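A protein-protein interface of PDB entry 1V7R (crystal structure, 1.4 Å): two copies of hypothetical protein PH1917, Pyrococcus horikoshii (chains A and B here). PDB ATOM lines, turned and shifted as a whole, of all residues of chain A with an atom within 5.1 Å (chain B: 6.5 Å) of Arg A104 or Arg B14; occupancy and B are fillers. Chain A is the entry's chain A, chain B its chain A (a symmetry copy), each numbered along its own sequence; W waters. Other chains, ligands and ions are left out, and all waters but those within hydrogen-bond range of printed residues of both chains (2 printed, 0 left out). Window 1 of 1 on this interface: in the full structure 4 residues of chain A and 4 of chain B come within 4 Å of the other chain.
The side-chain carboxylate (OE1) of Glu A149 lies within salt-bridge range of the guanidinium group (NH1) of Arg B14, 3.6 Å away. The indole nitrogen (NE1) of Trp A127 lies close to the guanidinium group (NE) of Arg B14.
OD1 of Asp A102 is in salt-bridge range of NE of Arg A104 (2.9 Å). O of Arg A104 sits at hydrogen-bond distance from N of Glu A71 (3.1 Å). The backbone carbonyl oxygen (O) of Trp A127 lies within hydrogen-bond range of the backbone NH (N) of Glu A149.
NH1 of Arg A104 touches CG of Arg B14, at 3.9 Å. Ala B17 touches Arg A104 (CB to NH2, 3.8 Å). Pro B10 touches Glu A149 (CB to OE1, 3.4 Å).
Arg A104 touches just these residues of chain B: Arg B14 (3.9 Å) and Ala B17 (3.8 Å). Of the printed residues of chain A, Arg B14 touches Arg A104, Trp A127 and Glu A149. Of the printed residues of chain B, Trp A127 touches Arg B14. Of the printed residues of chain B, Glu A149 touches Pro B10 (3.4 Å) and Arg B14 (3.6 Å). Val B13 touches none of the printed residues of chain A. Ser A72 touches none of the printed residues of chain B. The nearest residue of chain B that does not touch Arg A104 is Asn B18 (4.7 Å). The nearest printed residue of chain A that does not touch Arg B14 is Gly A128 (6.4 Å).
Printed residues of chain B that touch a printed residue of chain A: Pro B10, Arg B14 and Ala B17. Along chain B the printed residues that touch a printed residue of chain A span positions 10 to 17. Of the 14 printed residues of chain A, 3 touch a printed residue of chain B. Hydrophobic or aromatic side chains of chain A within 4 Å of the printed part of chain B: Trp A127. Among the printed residues, 5 pairs touch across the chains.
No position is printed for both chains. Of the 5 pairs that touch across the chains among the printed residues, none has its exchanged pair printed and touching as well.
Water W1 bridges O of Arg B14 (2.8 Å) and NH1 of Arg A104 (3.0 Å). Water W2 lies within hydrogen-bond range of OE1 of Glu A71 (3.1 Å) and ND2 of Asn B18 (3.1 Å).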
ATOM      1  N   PHE A  69      -7.447  -2.545  17.137  1.00  0.00           N
ATOM      2  CA  PHE A  69      -8.010  -1.222  16.866  1.00  0.00           C
ATOM      3  C   PHE A  69      -6.931  -0.320  16.264  1.00  0.00           C
ATOM      4  O   PHE A  69      -5.992   0.088  16.948  1.00  0.00           O
ATOM      5  CB  PHE A  69      -8.550  -0.622  18.174  1.00  0.00           C
ATOM      6  CG  PHE A  69      -9.645  -1.444  18.817  1.00  0.00           C
ATOM      7  CD1 PHE A  69     -10.971  -1.022  18.767  1.00  0.00           C
ATOM      8  CD2 PHE A  69      -9.348  -2.642  19.465  1.00  0.00           C
ATOM      9  CE1 PHE A  69     -11.985  -1.778  19.353  1.00  0.00           C
ATOM     10  CE2 PHE A  69     -10.357  -3.404  20.053  1.00  0.00           C
ATOM     11  CZ  PHE A  69     -11.675  -2.970  19.996  1.00  0.00           C
ATOM     12  N   ILE A  70      -7.072  -0.021  14.975  1.00  0.00           N
ATOM     13  CA  ILE A  70      -6.091   0.801  14.261  1.00  0.00           C
ATOM     14  C   ILE A  70      -6.463   2.283  14.257  1.00  0.00           C
ATOM     15  O   ILE A  70      -7.519   2.677  13.764  1.00  0.00           O
ATOM     16  CB  ILE A  70      -5.912   0.265  12.813  1.00  0.00           C
ATOM     17  CG1 ILE A  70      -5.487  -1.209  12.877  1.00  0.00           C
ATOM     18  CG2 ILE A  70      -4.868   1.092  12.059  1.00  0.00           C
ATOM     19  CD1 ILE A  70      -5.470  -1.915  11.540  1.00  0.00           C
ATOM     20  N   GLU A  71      -5.577   3.099  14.820  1.00  0.00           N
ATOM     21  CA  GLU A  71      -5.798   4.541  14.930  1.00  0.00           C
ATOM     22  C   GLU A  71      -6.195   5.265  13.647  1.00  0.00           C
ATOM     23  O   GLU A  71      -7.208   5.961  13.610  1.00  0.00           O
ATOM     24  CB  GLU A  71      -4.555   5.206  15.514  1.00  0.00           C
ATOM     25  CG  GLU A  71      -4.386   4.980  16.997  1.00  0.00           C
ATOM     26  CD  GLU A  71      -5.537   5.561  17.797  1.00  0.00           C
ATOM     27  OE1 GLU A  71      -5.765   6.787  17.713  1.00  0.00           O
ATOM     28  OE2 GLU A  71      -6.215   4.792  18.509  1.00  0.00           O
ATOM     29  N   SER A  72      -5.398   5.099  12.601  1.00  0.00           N
ATOM     30  CA  SER A  72      -5.666   5.761  11.330  1.00  0.00           C
ATOM     31  C   SER A  72      -6.952   5.283  10.667  1.00  0.00           C
ATOM     32  O   SER A  72      -7.428   5.898   9.712  1.00  0.00           O
ATOM     33  CB  SER A  72      -4.490   5.551  10.377  1.00  0.00           C
ATOM     34  OG  SER A  72      -4.292   4.175  10.116  1.00  0.00           O
ATOM     35  N   ASP A 102       0.581   7.409  10.273  1.00  0.00           N
ATOM     36  CA  ASP A 102       0.473   6.854  11.598  1.00  0.00           C
ATOM     37  C   ASP A 102       0.024   5.403  11.517  1.00  0.00           C
ATOM     38  O   ASP A 102      -1.099   5.099  11.086  1.00  0.00           O
ATOM     39  CB  ASP A 102      -0.546   7.685  12.360  1.00  0.00           C
ATOM     40  CG  ASP A 102      -0.880   7.107  13.699  1.00  0.00           C
ATOM     41  OD1 ASP A 102      -0.013   6.437  14.282  1.00  0.00           O
ATOM     42  OD2 ASP A 102      -2.010   7.349  14.179  1.00  0.00           O
ATOM     43  N   ARG A 103       0.913   4.509  11.933  1.00  0.00           N
ATOM     44  CA  ARG A 103       0.619   3.087  11.900  1.00  0.00           C
ATOM     45  C   ARG A 103       0.330   2.511  13.281  1.00  0.00           C
ATOM     46  O   ARG A 103       0.358   1.293  13.466  1.00  0.00           O
ATOM     47  CB  ARG A 103       1.786   2.333  11.261  1.00  0.00           C
ATOM     48  CG  ARG A 103       2.128   2.801   9.852  1.00  0.00           C
ATOM     49  CD  ARG A 103       3.199   1.924   9.220  1.00  0.00           C
ATOM     50  NE  ARG A 103       2.701   0.601   8.840  1.00  0.00           N
ATOM     51  CZ  ARG A 103       1.980   0.353   7.749  1.00  0.00           C
ATOM     52  NH1 ARG A 103       1.664   1.337   6.915  1.00  0.00           N
ATOM     53  NH2 ARG A 103       1.580  -0.883   7.484  1.00  0.00           N
ATOM     54  N   ARG A 104       0.040   3.373  14.247  1.00  0.00           N
ATOM     55  CA  ARG A 104      -0.242   2.907  15.598  1.00  0.00           C
ATOM     56  C   ARG A 104      -1.585   2.197  15.719  1.00  0.00           C
ATOM     57  O   ARG A 104      -2.546   2.502  15.012  1.00  0.00           O
ATOM     58  CB  ARG A 104      -0.191   4.071  16.581  1.00  0.00           C
ATOM     59  CG  ARG A 104       1.178   4.716  16.699  1.00  0.00           C
ATOM     60  CD  ARG A 104       1.096   5.923  17.601  1.00  0.00           C
ATOM     61  NE  ARG A 104       0.086   6.852  17.108  1.00  0.00           N
ATOM     62  CZ  ARG A 104      -0.802   7.466  17.880  1.00  0.00           C
ATOM     63  NH1 ARG A 104      -0.802   7.253  19.189  1.00  0.00           N
ATOM     64  NH2 ARG A 104      -1.708   8.266  17.338  1.00  0.00           N
ATOM     65  N   ALA A 105      -1.634   1.246  16.641  1.00  0.00           N
ATOM     66  CA  ALA A 105      -2.840   0.469  16.873  1.00  0.00           C
ATOM     67  C   ALA A 105      -2.717  -0.188  18.228  1.00  0.00           C
ATOM     68  O   ALA A 105      -1.637  -0.220  18.818  1.00  0.00           O
ATOM     69  CB  ALA A 105      -2.980  -0.607  15.792  1.00  0.00           C
ATOM     70  N   TYR A 106      -3.827  -0.711  18.728  1.00  0.00           N
ATOM     71  CA  TYR A 106      -3.769  -1.414  19.992  1.00  0.00           C
ATOM     72  C   TYR A 106      -4.656  -2.630  19.936  1.00  0.00           C
ATOM     73  O   TYR A 106      -5.633  -2.689  19.187  1.00  0.00           O
ATOM     74  CB  TYR A 106      -4.174  -0.518  21.175  1.00  0.00           C
ATOM     75  CG  TYR A 106      -5.621  -0.080  21.202  1.00  0.00           C
ATOM     76  CD1 TYR A 106      -6.620  -0.890  21.754  1.00  0.00           C
ATOM     77  CD2 TYR A 106      -5.991   1.156  20.676  1.00  0.00           C
ATOM     78  CE1 TYR A 106      -7.949  -0.470  21.783  1.00  0.00           C
ATOM     79  CE2 TYR A 106      -7.314   1.581  20.697  1.00  0.00           C
ATOM     80  CZ  TYR A 106      -8.290   0.766  21.254  1.00  0.00           C
ATOM     81  OH  TYR A 106      -9.593   1.205  21.291  1.00  0.00           O
ATOM     82  N   TRP A 127      -0.577  -1.394  23.261  1.00  0.00           N
ATOM     83  CA  TRP A 127      -0.387  -0.542  22.102  1.00  0.00           C
ATOM     84  C   TRP A 127       0.830  -1.011  21.321  1.00  0.00           C
ATOM     85  O   TRP A 127       1.731  -1.656  21.859  1.00  0.00           O
ATOM     86  CB  TRP A 127      -0.190   0.923  22.515  1.00  0.00           C
ATOM     87  CG  TRP A 127      -1.464   1.675  22.769  1.00  0.00           C
ATOM     88  CD1 TRP A 127      -2.199   1.693  23.923  1.00  0.00           C
ATOM     89  CD2 TRP A 127      -2.156   2.519  21.841  1.00  0.00           C
ATOM     90  NE1 TRP A 127      -3.302   2.500  23.767  1.00  0.00           N
ATOM     91  CE2 TRP A 127      -3.303   3.018  22.500  1.00  0.00           C
ATOM     92  CE3 TRP A 127      -1.920   2.901  20.513  1.00  0.00           C
ATOM     93  CZ2 TRP A 127      -4.207   3.883  21.877  1.00  0.00           C
ATOM     94  CZ3 TRP A 127      -2.823   3.763  19.894  1.00  0.00           C
ATOM     95  CH2 TRP A 127      -3.953   4.242  20.579  1.00  0.00           C
ATOM     96  N   GLY A 128       0.844  -0.681  20.039  1.00  0.00           N
ATOM     97  CA  GLY A 128       1.945  -1.071  19.188  1.00  0.00           C
ATOM     98  C   GLY A 128       1.760  -0.441  17.832  1.00  0.00           C
ATOM     99  O   GLY A 128       1.178   0.640  17.712  1.00  0.00           O
ATOM    100  N   ARG A 129       2.255  -1.110  16.804  1.00  0.00           N
ATOM    101  CA  ARG A 129       2.113  -0.586  15.459  1.00  0.00           C
ATOM    102  C   ARG A 129       1.952  -1.703  14.447  1.00  0.00           C
ATOM    103  O   ARG A 129       2.308  -2.858  14.702  1.00  0.00           O
ATOM    104  CB  ARG A 129       3.317   0.287  15.089  1.00  0.00           C
ATOM    105  CG  ARG A 129       4.628  -0.457  14.947  1.00  0.00           C
ATOM    106  CD  ARG A 129       5.726   0.491  14.476  1.00  0.00           C
ATOM    107  NE  ARG A 129       6.966  -0.202  14.132  1.00  0.00           N
ATOM    108  CZ  ARG A 129       7.772  -0.786  15.012  1.00  0.00           C
ATOM    109  NH1 ARG A 129       7.477  -0.764  16.304  1.00  0.00           N
ATOM    110  NH2 ARG A 129       8.876  -1.394  14.599  1.00  0.00           N
ATOM    111  N   ILE A 130       1.383  -1.348  13.304  1.00  0.00           N
ATOM    112  CA  ILE A 130       1.188  -2.293  12.222  1.00  0.00           C
ATOM    113  C   ILE A 130       2.464  -2.307  11.384  1.00  0.00           C
ATOM    114  O   ILE A 130       2.936  -1.263  10.932  1.00  0.00           O
ATOM    115  CB  ILE A 130      -0.008  -1.879  11.333  1.00  0.00           C
ATOM    116  CG1 ILE A 130      -1.270  -1.702  12.189  1.00  0.00           C
ATOM    117  CG2 ILE A 130      -0.230  -2.915  10.247  1.00  0.00           C
ATOM    118  CD1 ILE A 130      -1.669  -2.940  12.988  1.00  0.00           C
ATOM    119  N   GLU A 149       4.606  -2.218  21.443  1.00  0.00           N
ATOM    120  CA  GLU A 149       5.553  -1.177  21.820  1.00  0.00           C
ATOM    121  C   GLU A 149       6.683  -1.755  22.669  1.00  0.00           C
ATOM    122  O   GLU A 149       6.442  -2.518  23.604  1.00  0.00           O
ATOM    123  CB  GLU A 149       4.826  -0.068  22.583  1.00  0.00           C
ATOM    124  CG  GLU A 149       5.721   1.072  23.034  1.00  0.00           C
ATOM    125  CD  GLU A 149       4.929   2.250  23.564  1.00  0.00           C
ATOM    126  OE1 GLU A 149       4.064   2.041  24.442  1.00  0.00           O
ATOM    127  OE2 GLU A 149       5.173   3.386  23.101  1.00  0.00           O
ATOM    128  N   PHE B   5       8.689  15.060  19.709  1.00  0.00           N
ATOM    129  CA  PHE B   5       8.337  15.120  21.124  1.00  0.00           C
ATOM    130  C   PHE B   5       9.373  14.304  21.889  1.00  0.00           C
ATOM    131  O   PHE B   5       9.397  13.073  21.819  1.00  0.00           O
ATOM    132  CB  PHE B   5       6.912  14.561  21.300  1.00  0.00           C
ATOM    133  CG  PHE B   5       6.354  14.659  22.708  1.00  0.00           C
ATOM    134  CD1 PHE B   5       6.998  15.385  23.712  1.00  0.00           C
ATOM    135  CD2 PHE B   5       5.154  14.021  23.015  1.00  0.00           C
ATOM    136  CE1 PHE B   5       6.446  15.465  24.999  1.00  0.00           C
ATOM    137  CE2 PHE B   5       4.597  14.095  24.290  1.00  0.00           C
ATOM    138  CZ  PHE B   5       5.243  14.817  25.283  1.00  0.00           C
ATOM    139  N   ASN B   9       7.710   8.953  28.077  1.00  0.00           N
ATOM    140  CA  ASN B   9       6.380   8.594  28.560  1.00  0.00           C
ATOM    141  C   ASN B   9       5.437   8.288  27.393  1.00  0.00           C
ATOM    142  O   ASN B   9       4.913   9.194  26.750  1.00  0.00           O
ATOM    143  CB  ASN B   9       5.829   9.742  29.418  1.00  0.00           C
ATOM    144  CG  ASN B   9       4.571   9.361  30.182  1.00  0.00           C
ATOM    145  OD1 ASN B   9       3.735   8.606  29.683  1.00  0.00           O
ATOM    146  ND2 ASN B   9       4.439   9.867  31.401  1.00  0.00           N
ATOM    147  N   PRO B  10       5.206   6.993  27.111  1.00  0.00           N
ATOM    148  CA  PRO B  10       4.328   6.558  26.020  1.00  0.00           C
ATOM    149  C   PRO B  10       2.899   7.085  26.141  1.00  0.00           C
ATOM    150  O   PRO B  10       2.262   7.406  25.137  1.00  0.00           O
ATOM    151  CB  PRO B  10       4.401   5.034  26.108  1.00  0.00           C
ATOM    152  CG  PRO B  10       4.614   4.797  27.571  1.00  0.00           C
ATOM    153  CD  PRO B  10       5.649   5.840  27.915  1.00  0.00           C
ATOM    154  N   GLY B  11       2.405   7.172  27.370  1.00  0.00           N
ATOM    155  CA  GLY B  11       1.060   7.672  27.587  1.00  0.00           C
ATOM    156  C   GLY B  11       0.918   9.119  27.150  1.00  0.00           C
ATOM    157  O   GLY B  11      -0.088   9.501  26.555  1.00  0.00           O
ATOM    158  N   LYS B  12       1.926   9.930  27.450  1.00  0.00           N
ATOM    159  CA  LYS B  12       1.886  11.334  27.065  1.00  0.00           C
ATOM    160  C   LYS B  12       1.955  11.475  25.554  1.00  0.00           C
ATOM    161  O   LYS B  12       1.268  12.311  24.974  1.00  0.00           O
ATOM    162  CB  LYS B  12       3.032  12.111  27.719  1.00  0.00           C
ATOM    163  CG  LYS B  12       2.860  12.270  29.218  1.00  0.00           C
ATOM    164  CD  LYS B  12       3.823  13.286  29.810  1.00  0.00           C
ATOM    165  CE  LYS B  12       3.511  13.496  31.285  1.00  0.00           C
ATOM    166  NZ  LYS B  12       4.335  14.569  31.910  1.00  0.00           N
ATOM    167  N   VAL B  13       2.777  10.651  24.915  1.00  0.00           N
ATOM    168  CA  VAL B  13       2.892  10.707  23.462  1.00  0.00           C
ATOM    169  C   VAL B  13       1.527  10.431  22.834  1.00  0.00           C
ATOM    170  O   VAL B  13       1.100  11.147  21.934  1.00  0.00           O
ATOM    171  CB  VAL B  13       3.902   9.671  22.926  1.00  0.00           C
ATOM    172  CG1 VAL B  13       3.929   9.719  21.406  1.00  0.00           C
ATOM    173  CG2 VAL B  13       5.288   9.958  23.482  1.00  0.00           C
ATOM    174  N   ARG B  14       0.838   9.405  23.328  1.00  0.00           N
ATOM    175  CA  ARG B  14      -0.475   9.065  22.795  1.00  0.00           C
ATOM    176  C   ARG B  14      -1.494  10.187  22.946  1.00  0.00           C
ATOM    177  O   ARG B  14      -2.293  10.429  22.048  1.00  0.00           O
ATOM    178  CB  ARG B  14      -1.007   7.790  23.452  1.00  0.00           C
ATOM    179  CG  ARG B  14      -0.295   6.530  22.987  1.00  0.00           C
ATOM    180  CD  ARG B  14      -1.097   5.288  23.328  1.00  0.00           C
ATOM    181  NE  ARG B  14      -1.026   4.946  24.742  1.00  0.00           N
ATOM    182  CZ  ARG B  14      -0.043   4.242  25.292  1.00  0.00           C
ATOM    183  NH1 ARG B  14       0.956   3.796  24.543  1.00  0.00           N
ATOM    184  NH2 ARG B  14      -0.057   3.985  26.592  1.00  0.00           N
ATOM    185  N   GLU B  15      -1.470  10.881  24.082  1.00  0.00           N
ATOM    186  CA  GLU B  15      -2.407  11.977  24.295  1.00  0.00           C
ATOM    187  C   GLU B  15      -2.099  13.151  23.373  1.00  0.00           C
ATOM    188  O   GLU B  15      -3.003  13.750  22.787  1.00  0.00           O
ATOM    189  CB  GLU B  15      -2.386  12.411  25.766  1.00  0.00           C
ATOM    190  CG  GLU B  15      -3.129  11.430  26.671  1.00  0.00           C
ATOM    191  CD  GLU B  15      -3.035  11.761  28.147  1.00  0.00           C
ATOM    192  OE1 GLU B  15      -2.817  12.942  28.493  1.00  0.00           O
ATOM    193  OE2 GLU B  15      -3.201  10.830  28.958  1.00  0.00           O
ATOM    194  N   VAL B  16      -0.818  13.477  23.240  1.00  0.00           N
ATOM    195  CA  VAL B  16      -0.408  14.571  22.372  1.00  0.00           C
ATOM    196  C   VAL B  16      -0.673  14.231  20.901  1.00  0.00           C
ATOM    197  O   VAL B  16      -1.191  15.062  20.154  1.00  0.00           O
ATOM    198  CB  VAL B  16       1.086  14.898  22.595  1.00  0.00           C
ATOM    199  CG1 VAL B  16       1.564  15.945  21.594  1.00  0.00           C
ATOM    200  CG2 VAL B  16       1.283  15.406  24.020  1.00  0.00           C
ATOM    201  N   ALA B  17      -0.345  13.004  20.501  1.00  0.00           N
ATOM    202  CA  ALA B  17      -0.554  12.578  19.118  1.00  0.00           C
ATOM    203  C   ALA B  17      -2.038  12.558  18.759  1.00  0.00           C
ATOM    204  O   ALA B  17      -2.423  12.924  17.649  1.00  0.00           O
ATOM    205  CB  ALA B  17       0.057  11.201  18.900  1.00  0.00           C
ATOM    206  N   ASN B  18      -2.870  12.133  19.705  1.00  0.00           N
ATOM    207  CA  ASN B  18      -4.312  12.071  19.492  1.00  0.00           C
ATOM    208  C   ASN B  18      -4.896  13.454  19.229  1.00  0.00           C
ATOM    209  O   ASN B  18      -5.660  13.652  18.286  1.00  0.00           O
ATOM    210  CB  ASN B  18      -4.995  11.469  20.726  1.00  0.00           C
ATOM    211  CG  ASN B  18      -6.509  11.442  20.603  1.00  0.00           C
ATOM    212  OD1 ASN B  18      -7.208  12.267  21.195  1.00  0.00           O
ATOM    213  ND2 ASN B  18      -7.025  10.484  19.835  1.00  0.00           N
ATOM    214  N   PHE B  19      -4.530  14.411  20.071  1.00  0.00           N
ATOM    215  CA  PHE B  19      -5.040  15.768  19.946  1.00  0.00           C
ATOM    216  C   PHE B  19      -4.571  16.486  18.687  1.00  0.00           C
ATOM    217  O   PHE B  19      -5.383  16.983  17.908  1.00  0.00           O
ATOM    218  CB  PHE B  19      -4.652  16.577  21.188  1.00  0.00           C
ATOM    219  CG  PHE B  19      -5.210  17.972  21.207  1.00  0.00           C
ATOM    220  CD1 PHE B  19      -4.639  18.977  20.432  1.00  0.00           C
ATOM    221  CD2 PHE B  19      -6.318  18.278  21.989  1.00  0.00           C
ATOM    222  CE1 PHE B  19      -5.164  20.265  20.431  1.00  0.00           C
ATOM    223  CE2 PHE B  19      -6.851  19.564  21.997  1.00  0.00           C
ATOM    224  CZ  PHE B  19      -6.271  20.560  21.215  1.00  0.00           C
ATOM    225  N   GLY B 139      -5.421   5.878  30.930  1.00  0.00           N
ATOM    226  CA  GLY B 139      -4.447   6.826  31.433  1.00  0.00           C
ATOM    227  C   GLY B 139      -3.255   6.268  32.181  1.00  0.00           C
ATOM    228  O   GLY B 139      -2.878   5.108  32.028  1.00  0.00           O
ATOM    229  N   ILE B 160      -8.775   8.546  25.681  1.00  0.00           N
ATOM    230  CA  ILE B 160      -7.823   9.622  25.431  1.00  0.00           C
ATOM    231  C   ILE B 160      -8.536  10.871  24.912  1.00  0.00           C
ATOM    232  O   ILE B 160      -8.253  11.984  25.349  1.00  0.00           O
ATOM    233  CB  ILE B 160      -6.745   9.177  24.417  1.00  0.00           C
ATOM    234  CG1 ILE B 160      -5.861   8.098  25.047  1.00  0.00           C
ATOM    235  CG2 ILE B 160      -5.904  10.375  23.986  1.00  0.00           C
ATOM    236  CD1 ILE B 160      -4.824   7.519  24.102  1.00  0.00           C
ATOM    237  N   ASN B 164      -8.585  14.361  26.919  1.00  0.00           N
ATOM    238  CA  ASN B 164      -8.038  15.555  26.279  1.00  0.00           C
ATOM    239  C   ASN B 164      -9.028  16.710  26.250  1.00  0.00           C
ATOM    240  O   ASN B 164      -8.633  17.875  26.300  1.00  0.00           O
ATOM    241  CB  ASN B 164      -7.591  15.255  24.843  1.00  0.00           C
ATOM    242  CG  ASN B 164      -6.193  14.667  24.771  1.00  0.00           C
ATOM    243  OD1 ASN B 164      -5.422  14.748  25.723  1.00  0.00           O
ATOM    244  ND2 ASN B 164      -5.853  14.091  23.623  1.00  0.00           N
HETATM  245  O   HOH W   1      -3.268   8.512  20.234  1.00  0.00           O
HETATM  246  O   HOH W   2      -5.759   7.787  20.627  1.00  0.00           O
